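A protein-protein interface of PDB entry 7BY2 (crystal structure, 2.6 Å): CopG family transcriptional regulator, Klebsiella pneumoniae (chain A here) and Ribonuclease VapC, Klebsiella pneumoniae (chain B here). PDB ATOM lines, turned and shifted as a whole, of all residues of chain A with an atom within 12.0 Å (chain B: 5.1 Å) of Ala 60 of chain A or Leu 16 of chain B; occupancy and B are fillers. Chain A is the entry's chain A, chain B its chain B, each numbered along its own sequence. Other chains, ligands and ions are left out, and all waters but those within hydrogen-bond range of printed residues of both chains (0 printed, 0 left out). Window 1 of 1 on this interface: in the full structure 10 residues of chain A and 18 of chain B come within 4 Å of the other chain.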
ATOM      1  N   ASP A  51      30.129  34.004  16.986  1.00  0.00           N
ATOM      2  CA  ASP A  51      31.012  32.875  16.601  1.00  0.00           C
ATOM      3  C   ASP A  51      30.508  31.393  16.664  1.00  0.00           C
ATOM      4  O   ASP A  51      31.237  30.505  16.211  1.00  0.00           O
ATOM      5  CB  ASP A  51      32.324  32.949  17.394  1.00  0.00           C
ATOM      6  CG  ASP A  51      32.905  34.348  17.452  1.00  0.00           C
ATOM      7  OD1 ASP A  51      33.870  34.635  16.711  1.00  0.00           O
ATOM      8  OD2 ASP A  51      32.415  35.159  18.261  1.00  0.00           O
ATOM      9  N   ARG A  52      29.322  31.099  17.214  1.00  0.00           N
ATOM     10  CA  ARG A  52      28.687  29.792  16.977  1.00  0.00           C
ATOM     11  C   ARG A  52      28.192  30.045  15.564  1.00  0.00           C
ATOM     12  O   ARG A  52      28.275  29.196  14.681  1.00  0.00           O
ATOM     13  CB  ARG A  52      27.496  29.416  17.921  1.00  0.00           C
ATOM     14  CG  ARG A  52      27.615  29.421  19.502  1.00  0.00           C
ATOM     15  CD  ARG A  52      28.220  28.310  20.348  1.00  0.00           C
ATOM     16  NE  ARG A  52      28.028  28.771  21.729  1.00  0.00           N
ATOM     17  CZ  ARG A  52      28.887  29.540  22.399  1.00  0.00           C
ATOM     18  NH1 ARG A  52      30.031  29.908  21.837  1.00  0.00           N
ATOM     19  NH2 ARG A  52      28.607  29.935  23.636  1.00  0.00           N
ATOM     20  N   ALA A  53      27.695  31.266  15.379  1.00  0.00           N
ATOM     21  CA  ALA A  53      27.176  31.736  14.105  1.00  0.00           C
ATOM     22  C   ALA A  53      28.215  31.515  13.029  1.00  0.00           C
ATOM     23  O   ALA A  53      27.942  30.863  12.030  1.00  0.00           O
ATOM     24  CB  ALA A  53      26.797  33.186  14.196  1.00  0.00           C
ATOM     25  N   LYS A  54      29.434  31.978  13.286  1.00  0.00           N
ATOM     26  CA  LYS A  54      30.529  31.774  12.346  1.00  0.00           C
ATOM     27  C   LYS A  54      30.829  30.285  12.214  1.00  0.00           C
ATOM     28  O   LYS A  54      31.166  29.805  11.134  1.00  0.00           O
ATOM     29  CB  LYS A  54      31.783  32.544  12.783  1.00  0.00           C
ATOM     30  CG  LYS A  54      32.948  31.670  13.214  1.00  0.00           C
ATOM     31  CD  LYS A  54      34.180  32.491  13.529  1.00  0.00           C
ATOM     32  CE  LYS A  54      35.303  31.601  14.030  1.00  0.00           C
ATOM     33  NZ  LYS A  54      34.946  30.949  15.319  1.00  0.00           N
ATOM     34  N   ASP A  55      30.675  29.553  13.313  1.00  0.00           N
ATOM     35  CA  ASP A  55      30.922  28.119  13.309  1.00  0.00           C
ATOM     36  C   ASP A  55      29.792  27.387  12.598  1.00  0.00           C
ATOM     37  O   ASP A  55      30.034  26.442  11.847  1.00  0.00           O
ATOM     38  CB  ASP A  55      31.087  27.591  14.734  1.00  0.00           C
ATOM     39  CG  ASP A  55      32.507  27.729  15.243  1.00  0.00           C
ATOM     40  OD1 ASP A  55      33.201  28.677  14.821  1.00  0.00           O
ATOM     41  OD2 ASP A  55      32.934  26.883  16.057  1.00  0.00           O
ATOM     42  N   THR A  56      28.562  27.832  12.833  1.00  0.00           N
ATOM     43  CA  THR A  56      27.402  27.276  12.148  1.00  0.00           C
ATOM     44  C   THR A  56      27.520  27.497  10.645  1.00  0.00           C
ATOM     45  O   THR A  56      27.363  26.566   9.855  1.00  0.00           O
ATOM     46  CB  THR A  56      26.088  27.905  12.648  1.00  0.00           C
ATOM     47  OG1 THR A  56      25.980  27.736  14.068  1.00  0.00           O
ATOM     48  CG2 THR A  56      24.894  27.257  11.966  1.00  0.00           C
ATOM     49  N   ILE A  57      27.803  28.738  10.264  1.00  0.00           N
ATOM     50  CA  ILE A  57      27.939  29.121   8.862  1.00  0.00           C
ATOM     51  C   ILE A  57      29.074  28.374   8.164  1.00  0.00           C
ATOM     52  O   ILE A  57      28.888  27.822   7.079  1.00  0.00           O
ATOM     53  CB  ILE A  57      28.181  30.640   8.722  1.00  0.00           C
ATOM     54  CG1 ILE A  57      26.962  31.424   9.210  1.00  0.00           C
ATOM     55  CG2 ILE A  57      28.489  31.004   7.281  1.00  0.00           C
ATOM     56  CD1 ILE A  57      27.220  32.909   9.355  1.00  0.00           C
ATOM     57  N   SER A  58      30.246  28.357   8.795  1.00  0.00           N
ATOM     58  CA  SER A  58      31.428  27.734   8.205  1.00  0.00           C
ATOM     59  C   SER A  58      31.261  26.229   8.037  1.00  0.00           C
ATOM     60  O   SER A  58      31.778  25.642   7.086  1.00  0.00           O
ATOM     61  CB  SER A  58      32.665  28.023   9.057  1.00  0.00           C
ATOM     62  OG  SER A  58      32.852  29.417   9.228  1.00  0.00           O
ATOM     63  N   SER A  59      30.543  25.606   8.965  1.00  0.00           N
ATOM     64  CA  SER A  59      30.282  24.175   8.879  1.00  0.00           C
ATOM     65  C   SER A  59      29.225  23.894   7.818  1.00  0.00           C
ATOM     66  O   SER A  59      29.199  22.817   7.221  1.00  0.00           O
ATOM     67  CB  SER A  59      29.835  23.624  10.234  1.00  0.00           C
ATOM     68  OG  SER A  59      30.599  24.182  11.289  1.00  0.00           O
ATOM     69  N   ALA A  60      28.357  24.873   7.588  1.00  0.00           N
ATOM     70  CA  ALA A  60      27.277  24.732   6.618  1.00  0.00           C
ATOM     71  C   ALA A  60      27.757  24.949   5.185  1.00  0.00           C
ATOM     72  O   ALA A  60      27.162  24.429   4.242  1.00  0.00           O
ATOM     73  CB  ALA A  60      26.151  25.699   6.947  1.00  0.00           C
ATOM     74  N   LEU A  61      28.827  25.723   5.025  1.00  0.00           N
ATOM     75  CA  LEU A  61      29.354  26.031   3.700  1.00  0.00           C
ATOM     76  C   LEU A  61      29.851  24.773   2.994  1.00  0.00           C
ATOM     77  O   LEU A  61      30.692  24.047   3.523  1.00  0.00           O
ATOM     78  CB  LEU A  61      30.486  27.057   3.802  1.00  0.00           C
ATOM     79  CG  LEU A  61      31.162  27.468   2.493  1.00  0.00           C
ATOM     80  CD1 LEU A  61      30.262  28.395   1.695  1.00  0.00           C
ATOM     81  CD2 LEU A  61      32.509  28.125   2.764  1.00  0.00           C
ATOM     82  N   GLY A  62      29.332  24.527   1.795  1.00  0.00           N
ATOM     83  CA  GLY A  62      29.720  23.369   1.010  1.00  0.00           C
ATOM     84  C   GLY A  62      29.354  22.040   1.642  1.00  0.00           C
ATOM     85  O   GLY A  62      29.957  21.012   1.327  1.00  0.00           O
ATOM     86  N   LEU A  63      28.365  22.058   2.530  1.00  0.00           N
ATOM     87  CA  LEU A  63      27.948  20.857   3.250  1.00  0.00           C
ATOM     88  C   LEU A  63      27.440  19.775   2.303  1.00  0.00           C
ATOM     89  O   LEU A  63      27.707  18.589   2.500  1.00  0.00           O
ATOM     90  CB  LEU A  63      26.869  21.203   4.277  1.00  0.00           C
ATOM     91  CG  LEU A  63      26.192  20.032   4.993  1.00  0.00           C
ATOM     92  CD1 LEU A  63      27.200  19.252   5.823  1.00  0.00           C
ATOM     93  CD2 LEU A  63      25.042  20.523   5.859  1.00  0.00           C
ATOM     94  N   TRP A  64      26.711  20.191   1.273  1.00  0.00           N
ATOM     95  CA  TRP A  64      26.154  19.255   0.304  1.00  0.00           C
ATOM     96  C   TRP A  64      27.224  18.745  -0.654  1.00  0.00           C
ATOM     97  O   TRP A  64      27.200  19.049  -1.846  1.00  0.00           O
ATOM     98  CB  TRP A  64      25.017  19.914  -0.479  1.00  0.00           C
ATOM     99  CG  TRP A  64      23.826  20.242   0.362  1.00  0.00           C
ATOM    100  CD1 TRP A  64      23.603  19.862   1.655  1.00  0.00           C
ATOM    101  CD2 TRP A  64      22.686  21.021  -0.025  1.00  0.00           C
ATOM    102  NE1 TRP A  64      22.397  20.355   2.094  1.00  0.00           N
ATOM    103  CE2 TRP A  64      21.816  21.070   1.078  1.00  0.00           C
ATOM    104  CE3 TRP A  64      22.323  21.681  -1.204  1.00  0.00           C
ATOM    105  CZ2 TRP A  64      20.603  21.753   1.044  1.00  0.00           C
ATOM    106  CZ3 TRP A  64      21.117  22.358  -1.237  1.00  0.00           C
ATOM    107  CH2 TRP A  64      20.272  22.388  -0.122  1.00  0.00           C
ATOM    108  N   ILE B  12      20.073  32.150  -1.171  1.00  0.00           N
ATOM    109  CA  ILE B  12      21.329  32.338  -0.451  1.00  0.00           C
ATOM    110  C   ILE B  12      21.700  31.095   0.349  1.00  0.00           C
ATOM    111  O   ILE B  12      22.850  30.651   0.324  1.00  0.00           O
ATOM    112  CB  ILE B  12      21.254  33.549   0.494  1.00  0.00           C
ATOM    113  CG1 ILE B  12      21.268  34.840  -0.318  1.00  0.00           C
ATOM    114  CG2 ILE B  12      22.418  33.545   1.475  1.00  0.00           C
ATOM    115  CD1 ILE B  12      20.195  35.799   0.075  1.00  0.00           C
ATOM    116  N   LEU B  13      20.721  30.535   1.052  1.00  0.00           N
ATOM    117  CA  LEU B  13      20.942  29.333   1.845  1.00  0.00           C
ATOM    118  C   LEU B  13      21.367  28.174   0.951  1.00  0.00           C
ATOM    119  O   LEU B  13      22.260  27.406   1.305  1.00  0.00           O
ATOM    120  CB  LEU B  13      19.686  28.964   2.639  1.00  0.00           C
ATOM    121  CG  LEU B  13      19.460  29.712   3.958  1.00  0.00           C
ATOM    122  CD1 LEU B  13      19.052  31.159   3.724  1.00  0.00           C
ATOM    123  CD2 LEU B  13      18.426  28.999   4.812  1.00  0.00           C
ATOM    124  N   ILE B  14      20.732  28.063  -0.212  1.00  0.00           N
ATOM    125  CA  ILE B  14      21.114  27.060  -1.200  1.00  0.00           C
ATOM    126  C   ILE B  14      22.560  27.272  -1.634  1.00  0.00           C
ATOM    127  O   ILE B  14      23.331  26.319  -1.741  1.00  0.00           O
ATOM    128  CB  ILE B  14      20.192  27.096  -2.434  1.00  0.00           C
ATOM    129  CG1 ILE B  14      18.767  26.701  -2.044  1.00  0.00           C
ATOM    130  CG2 ILE B  14      20.709  26.166  -3.521  1.00  0.00           C
ATOM    131  CD1 ILE B  14      18.662  25.321  -1.432  1.00  0.00           C
ATOM    132  N   ASP B  15      22.924  28.530  -1.867  1.00  0.00           N
ATOM    133  CA  ASP B  15      24.290  28.888  -2.244  1.00  0.00           C
ATOM    134  C   ASP B  15      25.288  28.499  -1.158  1.00  0.00           C
ATOM    135  O   ASP B  15      26.351  27.951  -1.451  1.00  0.00           O
ATOM    136  CB  ASP B  15      24.395  30.386  -2.528  1.00  0.00           C
ATOM    137  CG  ASP B  15      23.797  30.770  -3.864  1.00  0.00           C
ATOM    138  OD1 ASP B  15      23.857  29.951  -4.804  1.00  0.00           O
ATOM    139  OD2 ASP B  15      23.265  31.892  -3.971  1.00  0.00           O
ATOM    140  N   LEU B  16      24.939  28.803   0.089  1.00  0.00           N
ATOM    141  CA  LEU B  16      25.763  28.452   1.241  1.00  0.00           C
ATOM    142  C   LEU B  16      26.083  26.964   1.261  1.00  0.00           C
ATOM    143  O   LEU B  16      27.246  26.568   1.188  1.00  0.00           O
ATOM    144  CB  LEU B  16      25.071  28.851   2.544  1.00  0.00           C
ATOM    145  CG  LEU B  16      25.832  28.465   3.814  1.00  0.00           C
ATOM    146  CD1 LEU B  16      27.058  29.349   4.004  1.00  0.00           C
ATOM    147  CD2 LEU B  16      24.922  28.519   5.029  1.00  0.00           C
ATOM    148  N   PHE B  17      25.039  26.146   1.367  1.00  0.00           N
ATOM    149  CA  PHE B  17      25.186  24.694   1.374  1.00  0.00           C
ATOM    150  C   PHE B  17      25.876  24.176   0.109  1.00  0.00           C
ATOM    151  O   PHE B  17      26.400  23.062   0.095  1.00  0.00           O
ATOM    152  CB  PHE B  17      23.819  24.019   1.534  1.00  0.00           C
ATOM    153  CG  PHE B  17      23.166  24.268   2.867  1.00  0.00           C
ATOM    154  CD1 PHE B  17      23.775  23.855   4.041  1.00  0.00           C
ATOM    155  CD2 PHE B  17      21.934  24.899   2.945  1.00  0.00           C
ATOM    156  CE1 PHE B  17      23.175  24.079   5.267  1.00  0.00           C
ATOM    157  CE2 PHE B  17      21.329  25.125   4.168  1.00  0.00           C
ATOM    158  CZ  PHE B  17      21.949  24.715   5.330  1.00  0.00           C
ATOM    159  N   SER B  18      25.872  24.983  -0.950  1.00  0.00           N
ATOM    160  CA  SER B  18      26.510  24.609  -2.208  1.00  0.00           C
ATOM    161  C   SER B  18      27.955  25.101  -2.292  1.00  0.00           C
ATOM    162  O   SER B  18      28.620  24.921  -3.313  1.00  0.00           O
ATOM    163  CB  SER B  18      25.712  25.148  -3.397  1.00  0.00           C
ATOM    164  OG  SER B  18      24.381  24.663  -3.376  1.00  0.00           O
ATOM    165  N   GLY B  19      28.434  25.721  -1.219  1.00  0.00           N
ATOM    166  CA  GLY B  19      29.822  26.145  -1.140  1.00  0.00           C
ATOM    167  C   GLY B  19      30.178  27.444  -1.837  1.00  0.00           C
ATOM    168  O   GLY B  19      31.266  27.575  -2.395  1.00  0.00           O
ATOM    169  N   ARG B  20      29.265  28.408  -1.806  1.00  0.00           N
ATOM    170  CA  ARG B  20      29.562  29.746  -2.299  1.00  0.00           C
ATOM    171  C   ARG B  20      30.002  30.630  -1.138  1.00  0.00           C
ATOM    172  O   ARG B  20      29.238  30.848  -0.198  1.00  0.00           O
ATOM    173  CB  ARG B  20      28.346  30.357  -2.998  1.00  0.00           C
ATOM    174  CG  ARG B  20      27.829  29.557  -4.181  1.00  0.00           C
ATOM    175  CD  ARG B  20      28.905  29.365  -5.238  1.00  0.00           C
ATOM    176  NE  ARG B  20      29.534  30.627  -5.619  1.00  0.00           N
ATOM    177  CZ  ARG B  20      30.419  30.751  -6.603  1.00  0.00           C
ATOM    178  NH1 ARG B  20      30.780  29.691  -7.311  1.00  0.00           N
ATOM    179  NH2 ARG B  20      30.941  31.938  -6.881  1.00  0.00           N
ATOM    180  N   ALA B  23      27.807  33.562  -0.118  1.00  0.00           N
ATOM    181  CA  ALA B  23      26.680  33.327   0.777  1.00  0.00           C
ATOM    182  C   ALA B  23      27.118  33.387   2.237  1.00  0.00           C
ATOM    183  O   ALA B  23      26.385  33.883   3.094  1.00  0.00           O
ATOM    184  CB  ALA B  23      26.033  31.989   0.474  1.00  0.00           C
ATOM    185  N   LYS B  24      28.315  32.877   2.509  1.00  0.00           N
ATOM    186  CA  LYS B  24      28.902  32.937   3.843  1.00  0.00           C
ATOM    187  C   LYS B  24      29.035  34.380   4.316  1.00  0.00           C
ATOM    188  O   LYS B  24      28.762  34.695   5.474  1.00  0.00           O
ATOM    189  CB  LYS B  24      30.269  32.245   3.852  1.00  0.00           C
ATOM    190  CG  LYS B  24      31.148  32.583   5.047  1.00  0.00           C
ATOM    191  CD  LYS B  24      32.487  31.866   4.956  1.00  0.00           C
ATOM    192  CE  LYS B  24      33.476  32.388   5.986  1.00  0.00           C
ATOM    193  NZ  LYS B  24      33.860  33.802   5.723  1.00  0.00           N
ATOM    194  N   LEU B  27      25.509  36.064   5.199  1.00  0.00           N
ATOM    195  CA  LEU B  27      25.022  35.724   6.532  1.00  0.00           C
ATOM    196  C   LEU B  27      25.826  36.430   7.618  1.00  0.00           C
ATOM    197  O   LEU B  27      25.266  36.906   8.606  1.00  0.00           O
ATOM    198  CB  LEU B  27      25.077  34.212   6.750  1.00  0.00           C
ATOM    199  CG  LEU B  27      24.242  33.334   5.821  1.00  0.00           C
ATOM    200  CD1 LEU B  27      24.495  31.876   6.137  1.00  0.00           C
ATOM    201  CD2 LEU B  27      22.765  33.656   5.958  1.00  0.00           C
ATOM    202  N   ALA B  60      21.642  22.887  11.103  1.00  0.00           N
ATOM    203  CA  ALA B  60      22.082  24.205  10.662  1.00  0.00           C
ATOM    204  C   ALA B  60      20.896  25.159  10.544  1.00  0.00           C
ATOM    205  O   ALA B  60      20.979  26.319  10.948  1.00  0.00           O
ATOM    206  CB  ALA B  60      22.820  24.105   9.336  1.00  0.00           C
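Of the 13 printed residues of chain B, 7 touch a printed residue of chain A. Hydrophobic or aromatic side chains of chain B within 4 Å of the printed part of chain A: Ile 14, Leu 16, Phe 17 and Leu 27. Hydrophobic or aromatic side chains of chain A within 4 Å of the printed part of chain B: Ile 57, Ala 60, Leu 61 and Trp 64. Among the printed residues, no Asp or Glu carboxylate lies within 4 Å of a Lys or Arg side-chain nitrogen of the other chain.
The backbone carbonyl oxygen (O) of Phe 17 of chain B lies within hydrogen-bond range of the backbone NH (N) of Leu 63 of chain A (3.3 Å). N of Gly 62 of chain A sits close to N of Gly 19 of chain B (3.4 Å). N of Trp 64 of chain A lies within hydrogen-bond range of O of Phe 17 of chain B. The backbone NH (N) of Gly 62 of chain A is in hydrogen-bond range of the backbone carbonyl oxygen (O) of Leu 16 of chain B (3.0 Å).
Of the printed residues of chain B, Ala 60 of chain A touches Leu 16 and Phe 17. Leu 16 of chain B touches four residues of chain A. No residue of chain A comes within 4 Å of Leu 13 of chain B. Of the printed residues of chain A, Ile 14 of chain B touches Trp 64 (3.6 Å). No residue of chain A comes within 4 Å of Asp 15 of chain B. Of chain A, only Ala 60 (3.4 Å), Gly 62 (3.5 Å), Leu 63 (3.3 Å) and Trp 64 (3.1 Å) come within 4 Å of Phe 17 of chain B. No residue of chain A comes within 4 Å of Ser 18 of chain B. Gly 19 of chain B touches just these residues of chain A: Leu 61 (3.6 Å) and Gly 62 (3.4 Å). No residue of chain A comes within 4 Å of Ala 23 of chain B. Printed residues of chain B within 4 Å of Ile 57 of chain A: Leu 16, Lys 24 and Leu 27. Printed residues of chain B within 4 Å of Leu 61 of chain A: Leu 16 (3.3 Å), Gly 19 (3.6 Å) and Arg 20 (3.3 Å). Of the printed residues of chain B, Gly 62 of chain A touches Leu 16 (3.0 Å), Phe 17 (3.5 Å) and Gly 19 (3.4 Å). Lys 54 of chain A touches none of the printed residues of chain B. Ser 58 of chain A touches none of the printed residues of chain B. The nearest residue of chain B that does not touch Ala 60 of chain A is Ala 60 of chain B (4.4 Å). The nearest printed residue of chain A that does not touch Arg 20 of chain B is Gly 62 of chain A (5.3 Å).
OG of Ser 18 of chain B sits at hydrogen-bond distance from O of Ile 14 of chain B (2.6 Å). The backbone NH (N) of Arg 20 of chain B sits at hydrogen-bond distance from the backbone carbonyl oxygen (O) of Asp 15 of chain B (3.0 Å).
Among the printed residues, merely in contact across the chains: Ile 57 of chain A with Leu 16 of chain B, Ile 57 of chain A with Lys 24 of chain B, Ile 57 of chain A with Leu 27 of chain B, Ala 60 of chain A with Leu 16 of chain B, Ala 60 of chain A with Phe 17 of chain B, Leu 61 of chain A with Leu 16 of chain B, Leu 61 of chain A with Gly 19 of chain B, Leu 61 of chain A with Arg 20 of chain B, Gly 62 of chain A with Phe 17 of chain B and Trp 64 of chain A with Ile 14 of chain B.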
